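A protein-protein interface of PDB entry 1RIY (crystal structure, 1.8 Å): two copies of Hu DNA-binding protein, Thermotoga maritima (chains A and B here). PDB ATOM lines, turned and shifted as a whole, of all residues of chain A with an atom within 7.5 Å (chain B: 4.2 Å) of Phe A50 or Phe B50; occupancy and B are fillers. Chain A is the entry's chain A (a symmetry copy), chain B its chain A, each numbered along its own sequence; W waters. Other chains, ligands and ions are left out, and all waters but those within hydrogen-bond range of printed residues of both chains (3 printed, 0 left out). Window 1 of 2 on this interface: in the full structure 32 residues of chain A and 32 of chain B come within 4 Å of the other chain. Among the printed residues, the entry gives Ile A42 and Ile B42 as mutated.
Water W2 bridges the backbone carbonyl oxygen of Phe A79 (2.9 Å) and the backbone NH of Phe B79 (3.0 Å).
Water W3 lies within hydrogen-bond range of O of Phe B79 (2.9 Å) and N of Phe A79 (3.0 Å).
Water W1 bridges the backbone NH (N) of Met A1 (2.9 Å) and the side-chain carboxylate (OE1) of Glu B40 (3.3 Å).
Among the printed residues, pairs that only touch across the chains: Met A1 with Ile B42 (3.4 Å), Leu A29 with Phe B47 (3.8 Å), Ile A32 with Phe B47 (3.9 Å), Phe A50 with Phe B50 (3.9 Å) and Phe A79 with Phe B79 (3.4 Å).
Of the 10 printed residues of chain B, 5 touch a printed residue of chain A.
Of the 24 printed residues of chain A, 5 touch a printed residue of chain B.
Among the printed residues, no Asp or Glu carboxylate lies within 4 Å of a Lys or Arg side-chain nitrogen of the other chain.
Phe B50 touches its own counterpart, Phe A50.
Phe B79 touches its own counterpart, Phe A79.
Positions printed for both chains: 36, 40, 41, 42, 47, 49, 50, 51, 78 and 79.
The backbone NH of Met A1 sits at hydrogen-bond distance from the backbone carbonyl oxygen of Lys B41 (2.7 Å).
Of the printed residues of chain B, Phe A50 touches Phe B50 (3.9 Å).
Of chain A, only Phe A50 (3.9 Å) comes within 4 Å of Phe B50.
Of the printed residues of chain B, Ile A32 touches Phe B47.
Of the printed residues of chain B, Phe A79 touches Phe B79.
Of the printed residues of chain B, Leu A29 touches Phe B47.
Printed residues of chain A within 4 Å of Phe B79: Phe A79.
Glu B51 touches none of the printed residues of chain A.
Leu A6 touches none of the printed residues of chain B.
The nearest residue of chain B that does not touch Phe A50 is Phe B47 (4.1 Å).
N of Phe B50 lies within hydrogen-bond range of O of Ile B42, 2.7 Å away.
O of Ile A42 lies within hydrogen-bond range of N of Phe A50.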
ATOM      1  N   MET A   1     -12.682 -43.443 -19.552  1.00  0.00           N
ATOM      2  CA  MET A   1     -13.727 -43.625 -20.645  1.00  0.00           C
ATOM      3  C   MET A   1     -13.493 -42.638 -21.808  1.00  0.00           C
ATOM      4  O   MET A   1     -13.357 -41.446 -21.568  1.00  0.00           O
ATOM      5  CB  MET A   1     -15.122 -43.362 -20.078  1.00  0.00           C
ATOM      6  CG  MET A   1     -16.266 -43.585 -21.013  1.00  0.00           C
ATOM      7  SD  MET A   1     -17.862 -43.235 -20.244  1.00  0.00           S
ATOM      8  CE  MET A   1     -17.898 -44.276 -18.806  1.00  0.00           C
ATOM      9  N   LEU A   6     -18.242 -44.083 -24.223  1.00  0.00           N
ATOM     10  CA  LEU A   6     -19.394 -43.275 -23.774  1.00  0.00           C
ATOM     11  C   LEU A   6     -20.595 -43.555 -24.664  1.00  0.00           C
ATOM     12  O   LEU A   6     -21.704 -43.804 -24.186  1.00  0.00           O
ATOM     13  CB  LEU A   6     -19.042 -41.793 -23.803  1.00  0.00           C
ATOM     14  CG  LEU A   6     -20.148 -40.796 -23.511  1.00  0.00           C
ATOM     15  CD1 LEU A   6     -20.726 -41.021 -22.099  1.00  0.00           C
ATOM     16  CD2 LEU A   6     -19.678 -39.344 -23.656  1.00  0.00           C
ATOM     17  N   LEU A  29     -22.516 -31.737 -28.583  1.00  0.00           N
ATOM     18  CA  LEU A  29     -21.185 -31.145 -28.462  1.00  0.00           C
ATOM     19  C   LEU A  29     -21.008 -29.952 -29.399  1.00  0.00           C
ATOM     20  O   LEU A  29     -20.427 -28.934 -29.019  1.00  0.00           O
ATOM     21  CB  LEU A  29     -20.110 -32.193 -28.734  1.00  0.00           C
ATOM     22  CG  LEU A  29     -20.117 -33.374 -27.749  1.00  0.00           C
ATOM     23  CD1 LEU A  29     -19.009 -34.310 -28.174  1.00  0.00           C
ATOM     24  CD2 LEU A  29     -19.912 -32.951 -26.334  1.00  0.00           C
ATOM     25  N   ILE A  32     -23.055 -26.938 -28.006  1.00  0.00           N
ATOM     26  CA  ILE A  32     -22.399 -26.334 -26.847  1.00  0.00           C
ATOM     27  C   ILE A  32     -21.181 -25.532 -27.328  1.00  0.00           C
ATOM     28  O   ILE A  32     -20.967 -24.361 -26.944  1.00  0.00           O
ATOM     29  CB  ILE A  32     -21.976 -27.403 -25.820  1.00  0.00           C
ATOM     30  CG1 ILE A  32     -23.201 -28.033 -25.155  1.00  0.00           C
ATOM     31  CG2 ILE A  32     -21.027 -26.781 -24.771  1.00  0.00           C
ATOM     32  CD1 ILE A  32     -22.892 -29.213 -24.321  1.00  0.00           C
ATOM     33  N   ALA A  35     -22.371 -22.363 -29.096  1.00  0.00           N
ATOM     34  CA  ALA A  35     -22.875 -21.391 -28.109  1.00  0.00           C
ATOM     35  C   ALA A  35     -21.715 -20.706 -27.336  1.00  0.00           C
ATOM     36  O   ALA A  35     -21.768 -19.486 -27.076  1.00  0.00           O
ATOM     37  CB  ALA A  35     -23.846 -22.056 -27.153  1.00  0.00           C
ATOM     38  N   LEU A  36     -20.689 -21.475 -26.965  1.00  0.00           N
ATOM     39  CA  LEU A  36     -19.535 -20.913 -26.279  1.00  0.00           C
ATOM     40  C   LEU A  36     -18.817 -19.928 -27.201  1.00  0.00           C
ATOM     41  O   LEU A  36     -18.357 -18.848 -26.759  1.00  0.00           O
ATOM     42  CB  LEU A  36     -18.562 -21.998 -25.864  1.00  0.00           C
ATOM     43  CG  LEU A  36     -19.082 -22.851 -24.698  1.00  0.00           C
ATOM     44  CD1 LEU A  36     -18.121 -24.058 -24.548  1.00  0.00           C
ATOM     45  CD2 LEU A  36     -19.166 -22.073 -23.442  1.00  0.00           C
ATOM     46  N   GLY A  39     -20.156 -16.685 -27.086  1.00  0.00           N
ATOM     47  CA  GLY A  39     -20.124 -16.095 -25.754  1.00  0.00           C
ATOM     48  C   GLY A  39     -21.293 -16.393 -24.851  1.00  0.00           C
ATOM     49  O   GLY A  39     -21.464 -15.730 -23.788  1.00  0.00           O
ATOM     50  N   GLU A  40     -22.112 -17.375 -25.231  1.00  0.00           N
ATOM     51  CA  GLU A  40     -23.273 -17.735 -24.425  1.00  0.00           C
ATOM     52  C   GLU A  40     -22.875 -18.662 -23.278  1.00  0.00           C
ATOM     53  O   GLU A  40     -21.760 -19.236 -23.282  1.00  0.00           O
ATOM     54  CB  GLU A  40     -24.346 -18.438 -25.286  1.00  0.00           C
ATOM     55  CG  GLU A  40     -24.944 -17.520 -26.339  1.00  0.00           C
ATOM     56  CD  GLU A  40     -25.961 -18.187 -27.227  1.00  0.00           C
ATOM     57  OE1 GLU A  40     -25.917 -19.412 -27.361  1.00  0.00           O
ATOM     58  OE2 GLU A  40     -26.772 -17.444 -27.845  1.00  0.00           O
ATOM     59  N   LYS A  41     -23.799 -18.782 -22.318  1.00  0.00           N
ATOM     60  CA  LYS A  41     -23.689 -19.710 -21.215  1.00  0.00           C
ATOM     61  C   LYS A  41     -24.591 -20.892 -21.539  1.00  0.00           C
ATOM     62  O   LYS A  41     -25.642 -20.683 -22.146  1.00  0.00           O
ATOM     63  CB  LYS A  41     -24.193 -18.978 -19.964  1.00  0.00           C
ATOM     64  CG  LYS A  41     -24.591 -19.830 -18.847  1.00  0.00           C
ATOM     65  CD  LYS A  41     -24.838 -18.968 -17.643  1.00  0.00           C
ATOM     66  N   ILE A  42     -24.161 -22.111 -21.194  1.00  0.00           N
ATOM     67  CA  ILE A  42     -24.959 -23.318 -21.341  1.00  0.00           C
ATOM     68  C   ILE A  42     -25.085 -23.886 -19.946  1.00  0.00           C
ATOM     69  O   ILE A  42     -24.108 -24.442 -19.426  1.00  0.00           O
ATOM     70  CB  ILE A  42     -24.332 -24.364 -22.254  1.00  0.00           C
ATOM     71  CG1 ILE A  42     -24.010 -23.772 -23.622  1.00  0.00           C
ATOM     72  CG2 ILE A  42     -25.326 -25.513 -22.449  1.00  0.00           C
ATOM     73  CD1 ILE A  42     -22.673 -23.120 -23.762  1.00  0.00           C
ATOM     74  N   GLN A  43     -26.271 -23.747 -19.359  1.00  0.00           N
ATOM     75  CA  GLN A  43     -26.520 -24.203 -17.996  1.00  0.00           C
ATOM     76  C   GLN A  43     -27.425 -25.386 -18.025  1.00  0.00           C
ATOM     77  O   GLN A  43     -28.494 -25.314 -18.568  1.00  0.00           O
ATOM     78  CB  GLN A  43     -27.111 -23.107 -17.131  1.00  0.00           C
ATOM     79  CG  GLN A  43     -26.999 -23.424 -15.638  1.00  0.00           C
ATOM     80  CD  GLN A  43     -26.728 -22.195 -14.840  1.00  0.00           C
ATOM     81  OE1 GLN A  43     -26.849 -21.088 -15.347  1.00  0.00           O
ATOM     82  NE2 GLN A  43     -26.390 -22.372 -13.598  1.00  0.00           N
ATOM     83  N   ILE A  44     -26.937 -26.497 -17.507  1.00  0.00           N
ATOM     84  CA  ILE A  44     -27.709 -27.718 -17.488  1.00  0.00           C
ATOM     85  C   ILE A  44     -28.039 -28.103 -16.065  1.00  0.00           C
ATOM     86  O   ILE A  44     -27.181 -28.577 -15.329  1.00  0.00           O
ATOM     87  CB  ILE A  44     -26.936 -28.866 -18.168  1.00  0.00           C
ATOM     88  CG1 ILE A  44     -26.643 -28.502 -19.624  1.00  0.00           C
ATOM     89  CG2 ILE A  44     -27.806 -30.106 -18.128  1.00  0.00           C
ATOM     90  CD1 ILE A  44     -25.578 -29.372 -20.320  1.00  0.00           C
ATOM     91  N   PHE A  47     -26.331 -30.773 -13.580  1.00  0.00           N
ATOM     92  CA  PHE A  47     -25.016 -31.145 -14.061  1.00  0.00           C
ATOM     93  C   PHE A  47     -24.046 -29.999 -13.838  1.00  0.00           C
ATOM     94  O   PHE A  47     -23.232 -30.056 -12.948  1.00  0.00           O
ATOM     95  CB  PHE A  47     -25.071 -31.561 -15.518  1.00  0.00           C
ATOM     96  CG  PHE A  47     -23.780 -32.131 -16.045  1.00  0.00           C
ATOM     97  CD1 PHE A  47     -23.337 -33.393 -15.669  1.00  0.00           C
ATOM     98  CD2 PHE A  47     -23.067 -31.457 -16.955  1.00  0.00           C
ATOM     99  CE1 PHE A  47     -22.158 -33.902 -16.166  1.00  0.00           C
ATOM    100  CE2 PHE A  47     -21.879 -31.962 -17.451  1.00  0.00           C
ATOM    101  CZ  PHE A  47     -21.432 -33.193 -17.047  1.00  0.00           C
ATOM    102  N   GLY A  48     -24.183 -28.923 -14.597  1.00  0.00           N
ATOM    103  CA  GLY A  48     -23.299 -27.764 -14.467  1.00  0.00           C
ATOM    104  C   GLY A  48     -23.468 -26.730 -15.568  1.00  0.00           C
ATOM    105  O   GLY A  48     -24.388 -26.879 -16.399  1.00  0.00           O
ATOM    106  N   SER A  49     -22.594 -25.722 -15.606  1.00  0.00           N
ATOM    107  CA  SER A  49     -22.701 -24.703 -16.625  1.00  0.00           C
ATOM    108  C   SER A  49     -21.358 -24.556 -17.363  1.00  0.00           C
ATOM    109  O   SER A  49     -20.273 -24.629 -16.757  1.00  0.00           O
ATOM    110  CB  SER A  49     -23.166 -23.368 -16.012  1.00  0.00           C
ATOM    111  OG  SER A  49     -22.163 -22.869 -15.178  1.00  0.00           O
ATOM    112  N   PHE A  50     -21.473 -24.347 -18.667  1.00  0.00           N
ATOM    113  CA  PHE A  50     -20.344 -24.052 -19.526  1.00  0.00           C
ATOM    114  C   PHE A  50     -20.406 -22.556 -19.898  1.00  0.00           C
ATOM    115  O   PHE A  50     -21.482 -22.008 -20.256  1.00  0.00           O
ATOM    116  CB  PHE A  50     -20.419 -24.909 -20.790  1.00  0.00           C
ATOM    117  CG  PHE A  50     -20.279 -26.377 -20.555  1.00  0.00           C
ATOM    118  CD1 PHE A  50     -21.398 -27.189 -20.446  1.00  0.00           C
ATOM    119  CD2 PHE A  50     -19.019 -26.955 -20.467  1.00  0.00           C
ATOM    120  CE1 PHE A  50     -21.270 -28.542 -20.229  1.00  0.00           C
ATOM    121  CE2 PHE A  50     -18.888 -28.321 -20.272  1.00  0.00           C
ATOM    122  CZ  PHE A  50     -19.997 -29.104 -20.166  1.00  0.00           C
ATOM    123  N   GLU A  51     -19.276 -21.862 -19.768  1.00  0.00           N
ATOM    124  CA  GLU A  51     -19.213 -20.471 -20.137  1.00  0.00           C
ATOM    125  C   GLU A  51     -17.784 -20.110 -20.493  1.00  0.00           C
ATOM    126  O   GLU A  51     -16.851 -20.840 -20.167  1.00  0.00           O
ATOM    127  CB  GLU A  51     -19.726 -19.580 -18.998  1.00  0.00           C
ATOM    128  CG  GLU A  51     -19.991 -18.142 -19.424  1.00  0.00           C
ATOM    129  CD  GLU A  51     -20.786 -17.357 -18.389  1.00  0.00           C
ATOM    130  OE1 GLU A  51     -21.041 -16.145 -18.601  1.00  0.00           O
ATOM    131  OE2 GLU A  51     -21.137 -17.951 -17.347  1.00  0.00           O
ATOM    132  N   VAL A  52     -17.634 -19.033 -21.236  1.00  0.00           N
ATOM    133  CA  VAL A  52     -16.321 -18.562 -21.625  1.00  0.00           C
ATOM    134  C   VAL A  52     -15.949 -17.440 -20.681  1.00  0.00           C
ATOM    135  O   VAL A  52     -16.781 -16.600 -20.355  1.00  0.00           O
ATOM    136  CB  VAL A  52     -16.331 -18.072 -23.075  1.00  0.00           C
ATOM    137  CG1 VAL A  52     -15.032 -17.413 -23.432  1.00  0.00           C
ATOM    138  CG2 VAL A  52     -16.586 -19.219 -23.995  1.00  0.00           C
ATOM    139  N   PRO A  77     -12.801 -21.524 -22.298  1.00  0.00           N
ATOM    140  CA  PRO A  77     -14.010 -22.206 -21.870  1.00  0.00           C
ATOM    141  C   PRO A  77     -13.830 -22.693 -20.462  1.00  0.00           C
ATOM    142  O   PRO A  77     -12.707 -23.083 -20.117  1.00  0.00           O
ATOM    143  CB  PRO A  77     -14.080 -23.425 -22.801  1.00  0.00           C
ATOM    144  CG  PRO A  77     -12.947 -23.344 -23.665  1.00  0.00           C
ATOM    145  CD  PRO A  77     -11.982 -22.364 -23.178  1.00  0.00           C
ATOM    146  N   LYS A  78     -14.897 -22.668 -19.671  1.00  0.00           N
ATOM    147  CA  LYS A  78     -14.871 -23.076 -18.277  1.00  0.00           C
ATOM    148  C   LYS A  78     -16.135 -23.833 -17.962  1.00  0.00           C
ATOM    149  O   LYS A  78     -17.214 -23.529 -18.523  1.00  0.00           O
ATOM    150  CB  LYS A  78     -14.812 -21.855 -17.343  1.00  0.00           C
ATOM    151  CG  LYS A  78     -15.120 -22.157 -15.857  1.00  0.00           C
ATOM    152  CD  LYS A  78     -15.163 -20.875 -14.989  1.00  0.00           C
ATOM    153  CE  LYS A  78     -14.513 -21.090 -13.621  1.00  0.00           C
ATOM    154  NZ  LYS A  78     -14.385 -19.820 -12.860  1.00  0.00           N
ATOM    155  N   PHE A  79     -16.018 -24.785 -17.042  1.00  0.00           N
ATOM    156  CA  PHE A  79     -17.155 -25.576 -16.589  1.00  0.00           C
ATOM    157  C   PHE A  79     -17.296 -25.415 -15.107  1.00  0.00           C
ATOM    158  O   PHE A  79     -16.321 -25.590 -14.360  1.00  0.00           O
ATOM    159  CB  PHE A  79     -17.012 -27.053 -16.937  1.00  0.00           C
ATOM    160  CG  PHE A  79     -18.056 -27.948 -16.321  1.00  0.00           C
ATOM    161  CD1 PHE A  79     -19.347 -27.993 -16.826  1.00  0.00           C
ATOM    162  CD2 PHE A  79     -17.740 -28.774 -15.253  1.00  0.00           C
ATOM    163  CE1 PHE A  79     -20.311 -28.852 -16.254  1.00  0.00           C
ATOM    164  CE2 PHE A  79     -18.720 -29.636 -14.699  1.00  0.00           C
ATOM    165  CZ  PHE A  79     -19.982 -29.654 -15.219  1.00  0.00           C
ATOM    166  N   LYS A  80     -18.481 -25.038 -14.671  1.00  0.00           N
ATOM    167  CA  LYS A  80     -18.778 -24.928 -13.249  1.00  0.00           C
ATOM    168  C   LYS A  80     -19.776 -26.015 -12.872  1.00  0.00           C
ATOM    169  O   LYS A  80     -20.940 -25.948 -13.260  1.00  0.00           O
ATOM    170  CB  LYS A  80     -19.371 -23.569 -12.878  1.00  0.00           C
ATOM    171  CG  LYS A  80     -18.528 -22.407 -13.292  1.00  0.00           C
ATOM    172  N   PRO A  81     -19.325 -27.002 -12.102  1.00  0.00           N
ATOM    173  CA  PRO A  81     -20.202 -28.106 -11.707  1.00  0.00           C
ATOM    174  C   PRO A  81     -21.299 -27.594 -10.827  1.00  0.00           C
ATOM    175  O   PRO A  81     -21.050 -26.718  -9.969  1.00  0.00           O
ATOM    176  CB  PRO A  81     -19.276 -29.061 -10.919  1.00  0.00           C
ATOM    177  CG  PRO A  81     -18.020 -28.349 -10.679  1.00  0.00           C
ATOM    178  CD  PRO A  81     -17.967 -27.155 -11.581  1.00  0.00           C
ATOM    179  N   LEU A  85     -23.977 -32.451  -8.727  1.00  0.00           N
ATOM    180  CA  LEU A  85     -22.748 -33.135  -9.157  1.00  0.00           C
ATOM    181  C   LEU A  85     -21.631 -32.993  -8.115  1.00  0.00           C
ATOM    182  O   LEU A  85     -20.891 -33.942  -7.838  1.00  0.00           O
ATOM    183  CB  LEU A  85     -22.274 -32.583 -10.521  1.00  0.00           C
ATOM    184  CG  LEU A  85     -21.019 -33.174 -11.160  1.00  0.00           C
ATOM    185  CD1 LEU A  85     -21.150 -34.673 -11.366  1.00  0.00           C
ATOM    186  CD2 LEU A  85     -20.710 -32.479 -12.466  1.00  0.00           C
ATOM    187  N   LEU B  36     -17.628 -40.250 -12.960  1.00  0.00           N
ATOM    188  CA  LEU B  36     -16.906 -39.340 -12.083  1.00  0.00           C
ATOM    189  C   LEU B  36     -16.999 -39.834 -10.640  1.00  0.00           C
ATOM    190  O   LEU B  36     -16.008 -39.776  -9.873  1.00  0.00           O
ATOM    191  CB  LEU B  36     -17.475 -37.938 -12.161  1.00  0.00           C
ATOM    192  CG  LEU B  36     -17.143 -37.232 -13.484  1.00  0.00           C
ATOM    193  CD1 LEU B  36     -17.984 -35.931 -13.533  1.00  0.00           C
ATOM    194  CD2 LEU B  36     -15.696 -36.942 -13.605  1.00  0.00           C
ATOM    195  N   GLU B  40     -13.401 -42.150 -12.357  1.00  0.00           N
ATOM    196  CA  GLU B  40     -12.908 -42.314 -13.720  1.00  0.00           C
ATOM    197  C   GLU B  40     -12.763 -40.961 -14.416  1.00  0.00           C
ATOM    198  O   GLU B  40     -13.306 -39.939 -13.934  1.00  0.00           O
ATOM    199  CB  GLU B  40     -13.863 -43.202 -14.550  1.00  0.00           C
ATOM    200  CG  GLU B  40     -13.918 -44.633 -14.041  1.00  0.00           C
ATOM    201  CD  GLU B  40     -14.876 -45.515 -14.798  1.00  0.00           C
ATOM    202  OE1 GLU B  40     -15.811 -44.989 -15.407  1.00  0.00           O
ATOM    203  OE2 GLU B  40     -14.708 -46.763 -14.716  1.00  0.00           O
ATOM    204  N   LYS B  41     -12.028 -40.990 -15.533  1.00  0.00           N
ATOM    205  CA  LYS B  41     -11.878 -39.857 -16.418  1.00  0.00           C
ATOM    206  C   LYS B  41     -12.793 -40.101 -17.609  1.00  0.00           C
ATOM    207  O   LYS B  41     -12.948 -41.256 -18.007  1.00  0.00           O
ATOM    208  CB  LYS B  41     -10.411 -39.834 -16.867  1.00  0.00           C
ATOM    209  CG  LYS B  41     -10.130 -39.074 -18.081  1.00  0.00           C
ATOM    210  CD  LYS B  41      -8.643 -38.962 -18.252  1.00  0.00           C
ATOM    211  N   ILE B  42     -13.431 -39.045 -18.126  1.00  0.00           N
ATOM    212  CA  ILE B  42     -14.249 -39.107 -19.327  1.00  0.00           C
ATOM    213  C   ILE B  42     -13.612 -38.137 -20.296  1.00  0.00           C
ATOM    214  O   ILE B  42     -13.746 -36.919 -20.113  1.00  0.00           O
ATOM    215  CB  ILE B  42     -15.702 -38.709 -19.103  1.00  0.00           C
ATOM    216  CG1 ILE B  42     -16.331 -39.541 -17.990  1.00  0.00           C
ATOM    217  CG2 ILE B  42     -16.491 -38.958 -20.393  1.00  0.00           C
ATOM    218  CD1 ILE B  42     -16.169 -39.017 -16.600  1.00  0.00           C
ATOM    219  N   PHE B  47     -13.530 -32.164 -27.632  1.00  0.00           N
ATOM    220  CA  PHE B  47     -14.306 -31.368 -26.702  1.00  0.00           C
ATOM    221  C   PHE B  47     -13.497 -31.118 -25.443  1.00  0.00           C
ATOM    222  O   PHE B  47     -13.003 -30.036 -25.242  1.00  0.00           O
ATOM    223  CB  PHE B  47     -15.633 -32.037 -26.396  1.00  0.00           C
ATOM    224  CG  PHE B  47     -16.573 -31.192 -25.577  1.00  0.00           C
ATOM    225  CD1 PHE B  47     -17.219 -30.089 -26.122  1.00  0.00           C
ATOM    226  CD2 PHE B  47     -16.868 -31.537 -24.318  1.00  0.00           C
ATOM    227  CE1 PHE B  47     -18.082 -29.331 -25.361  1.00  0.00           C
ATOM    228  CE2 PHE B  47     -17.728 -30.775 -23.549  1.00  0.00           C
ATOM    229  CZ  PHE B  47     -18.333 -29.668 -24.085  1.00  0.00           C
ATOM    230  N   SER B  49     -12.062 -33.131 -21.269  1.00  0.00           N
ATOM    231  CA  SER B  49     -12.091 -34.256 -20.362  1.00  0.00           C
ATOM    232  C   SER B  49     -12.704 -33.830 -19.016  1.00  0.00           C
ATOM    233  O   SER B  49     -12.462 -32.716 -18.516  1.00  0.00           O
ATOM    234  CB  SER B  49     -10.679 -34.848 -20.187  1.00  0.00           C
ATOM    235  OG  SER B  49      -9.874 -33.928 -19.513  1.00  0.00           O
ATOM    236  N   PHE B  50     -13.487 -34.744 -18.461  1.00  0.00           N
ATOM    237  CA  PHE B  50     -14.058 -34.601 -17.137  1.00  0.00           C
ATOM    238  C   PHE B  50     -13.302 -35.553 -16.187  1.00  0.00           C
ATOM    239  O   PHE B  50     -13.043 -36.742 -16.510  1.00  0.00           O
ATOM    240  CB  PHE B  50     -15.542 -34.967 -17.172  1.00  0.00           C
ATOM    241  CG  PHE B  50     -16.388 -34.054 -17.996  1.00  0.00           C
ATOM    242  CD1 PHE B  50     -16.712 -34.373 -19.306  1.00  0.00           C
ATOM    243  CD2 PHE B  50     -16.886 -32.878 -17.449  1.00  0.00           C
ATOM    244  CE1 PHE B  50     -17.491 -33.532 -20.066  1.00  0.00           C
ATOM    245  CE2 PHE B  50     -17.691 -32.040 -18.206  1.00  0.00           C
ATOM    246  CZ  PHE B  50     -17.998 -32.369 -19.491  1.00  0.00           C
ATOM    247  N   GLU B  51     -12.888 -35.035 -15.030  1.00  0.00           N
ATOM    248  CA  GLU B  51     -12.218 -35.851 -14.050  1.00  0.00           C
ATOM    249  C   GLU B  51     -12.422 -35.250 -12.672  1.00  0.00           C
ATOM    250  O   GLU B  51     -12.807 -34.091 -12.543  1.00  0.00           O
ATOM    251  CB  GLU B  51     -10.722 -35.971 -14.370  1.00  0.00           C
ATOM    252  CG  GLU B  51     -10.017 -37.063 -13.577  1.00  0.00           C
ATOM    253  CD  GLU B  51      -8.630 -37.384 -14.119  1.00  0.00           C
ATOM    254  OE1 GLU B  51      -7.925 -38.243 -13.532  1.00  0.00           O
ATOM    255  OE2 GLU B  51      -8.235 -36.755 -15.124  1.00  0.00           O
ATOM    256  N   LYS B  78     -13.953 -31.629 -12.366  1.00  0.00           N
ATOM    257  CA  LYS B  78     -13.228 -30.632 -13.134  1.00  0.00           C
ATOM    258  C   LYS B  78     -13.346 -30.959 -14.600  1.00  0.00           C
ATOM    259  O   LYS B  78     -13.399 -32.151 -14.983  1.00  0.00           O
ATOM    260  CB  LYS B  78     -11.733 -30.634 -12.772  1.00  0.00           C
ATOM    261  CG  LYS B  78     -10.825 -29.860 -13.758  1.00  0.00           C
ATOM    262  CD  LYS B  78      -9.321 -29.997 -13.410  1.00  0.00           C
ATOM    263  CE  LYS B  78      -8.568 -28.681 -13.608  1.00  0.00           C
ATOM    264  NZ  LYS B  78      -7.173 -28.756 -13.101  1.00  0.00           N
ATOM    265  N   PHE B  79     -13.344 -29.914 -15.421  1.00  0.00           N
ATOM    266  CA  PHE B  79     -13.402 -30.060 -16.870  1.00  0.00           C
ATOM    267  C   PHE B  79     -12.204 -29.392 -17.471  1.00  0.00           C
ATOM    268  O   PHE B  79     -11.916 -28.226 -17.165  1.00  0.00           O
ATOM    269  CB  PHE B  79     -14.676 -29.471 -17.465  1.00  0.00           C
ATOM    270  CG  PHE B  79     -14.699 -29.413 -18.970  1.00  0.00           C
ATOM    271  CD1 PHE B  79     -14.921 -30.555 -19.725  1.00  0.00           C
ATOM    272  CD2 PHE B  79     -14.532 -28.208 -19.635  1.00  0.00           C
ATOM    273  CE1 PHE B  79     -14.963 -30.485 -21.135  1.00  0.00           C
ATOM    274  CE2 PHE B  79     -14.587 -28.158 -21.051  1.00  0.00           C
ATOM    275  CZ  PHE B  79     -14.805 -29.301 -21.765  1.00  0.00           C
HETATM  276  O   HOH W   1     -13.509 -45.518 -17.684  1.00  0.00           O
HETATM  277  O   HOH W   2     -13.997 -27.315 -14.135  1.00  0.00           O
HETATM  278  O   HOH W   3     -13.237 -25.714 -16.555  1.00  0.00           O
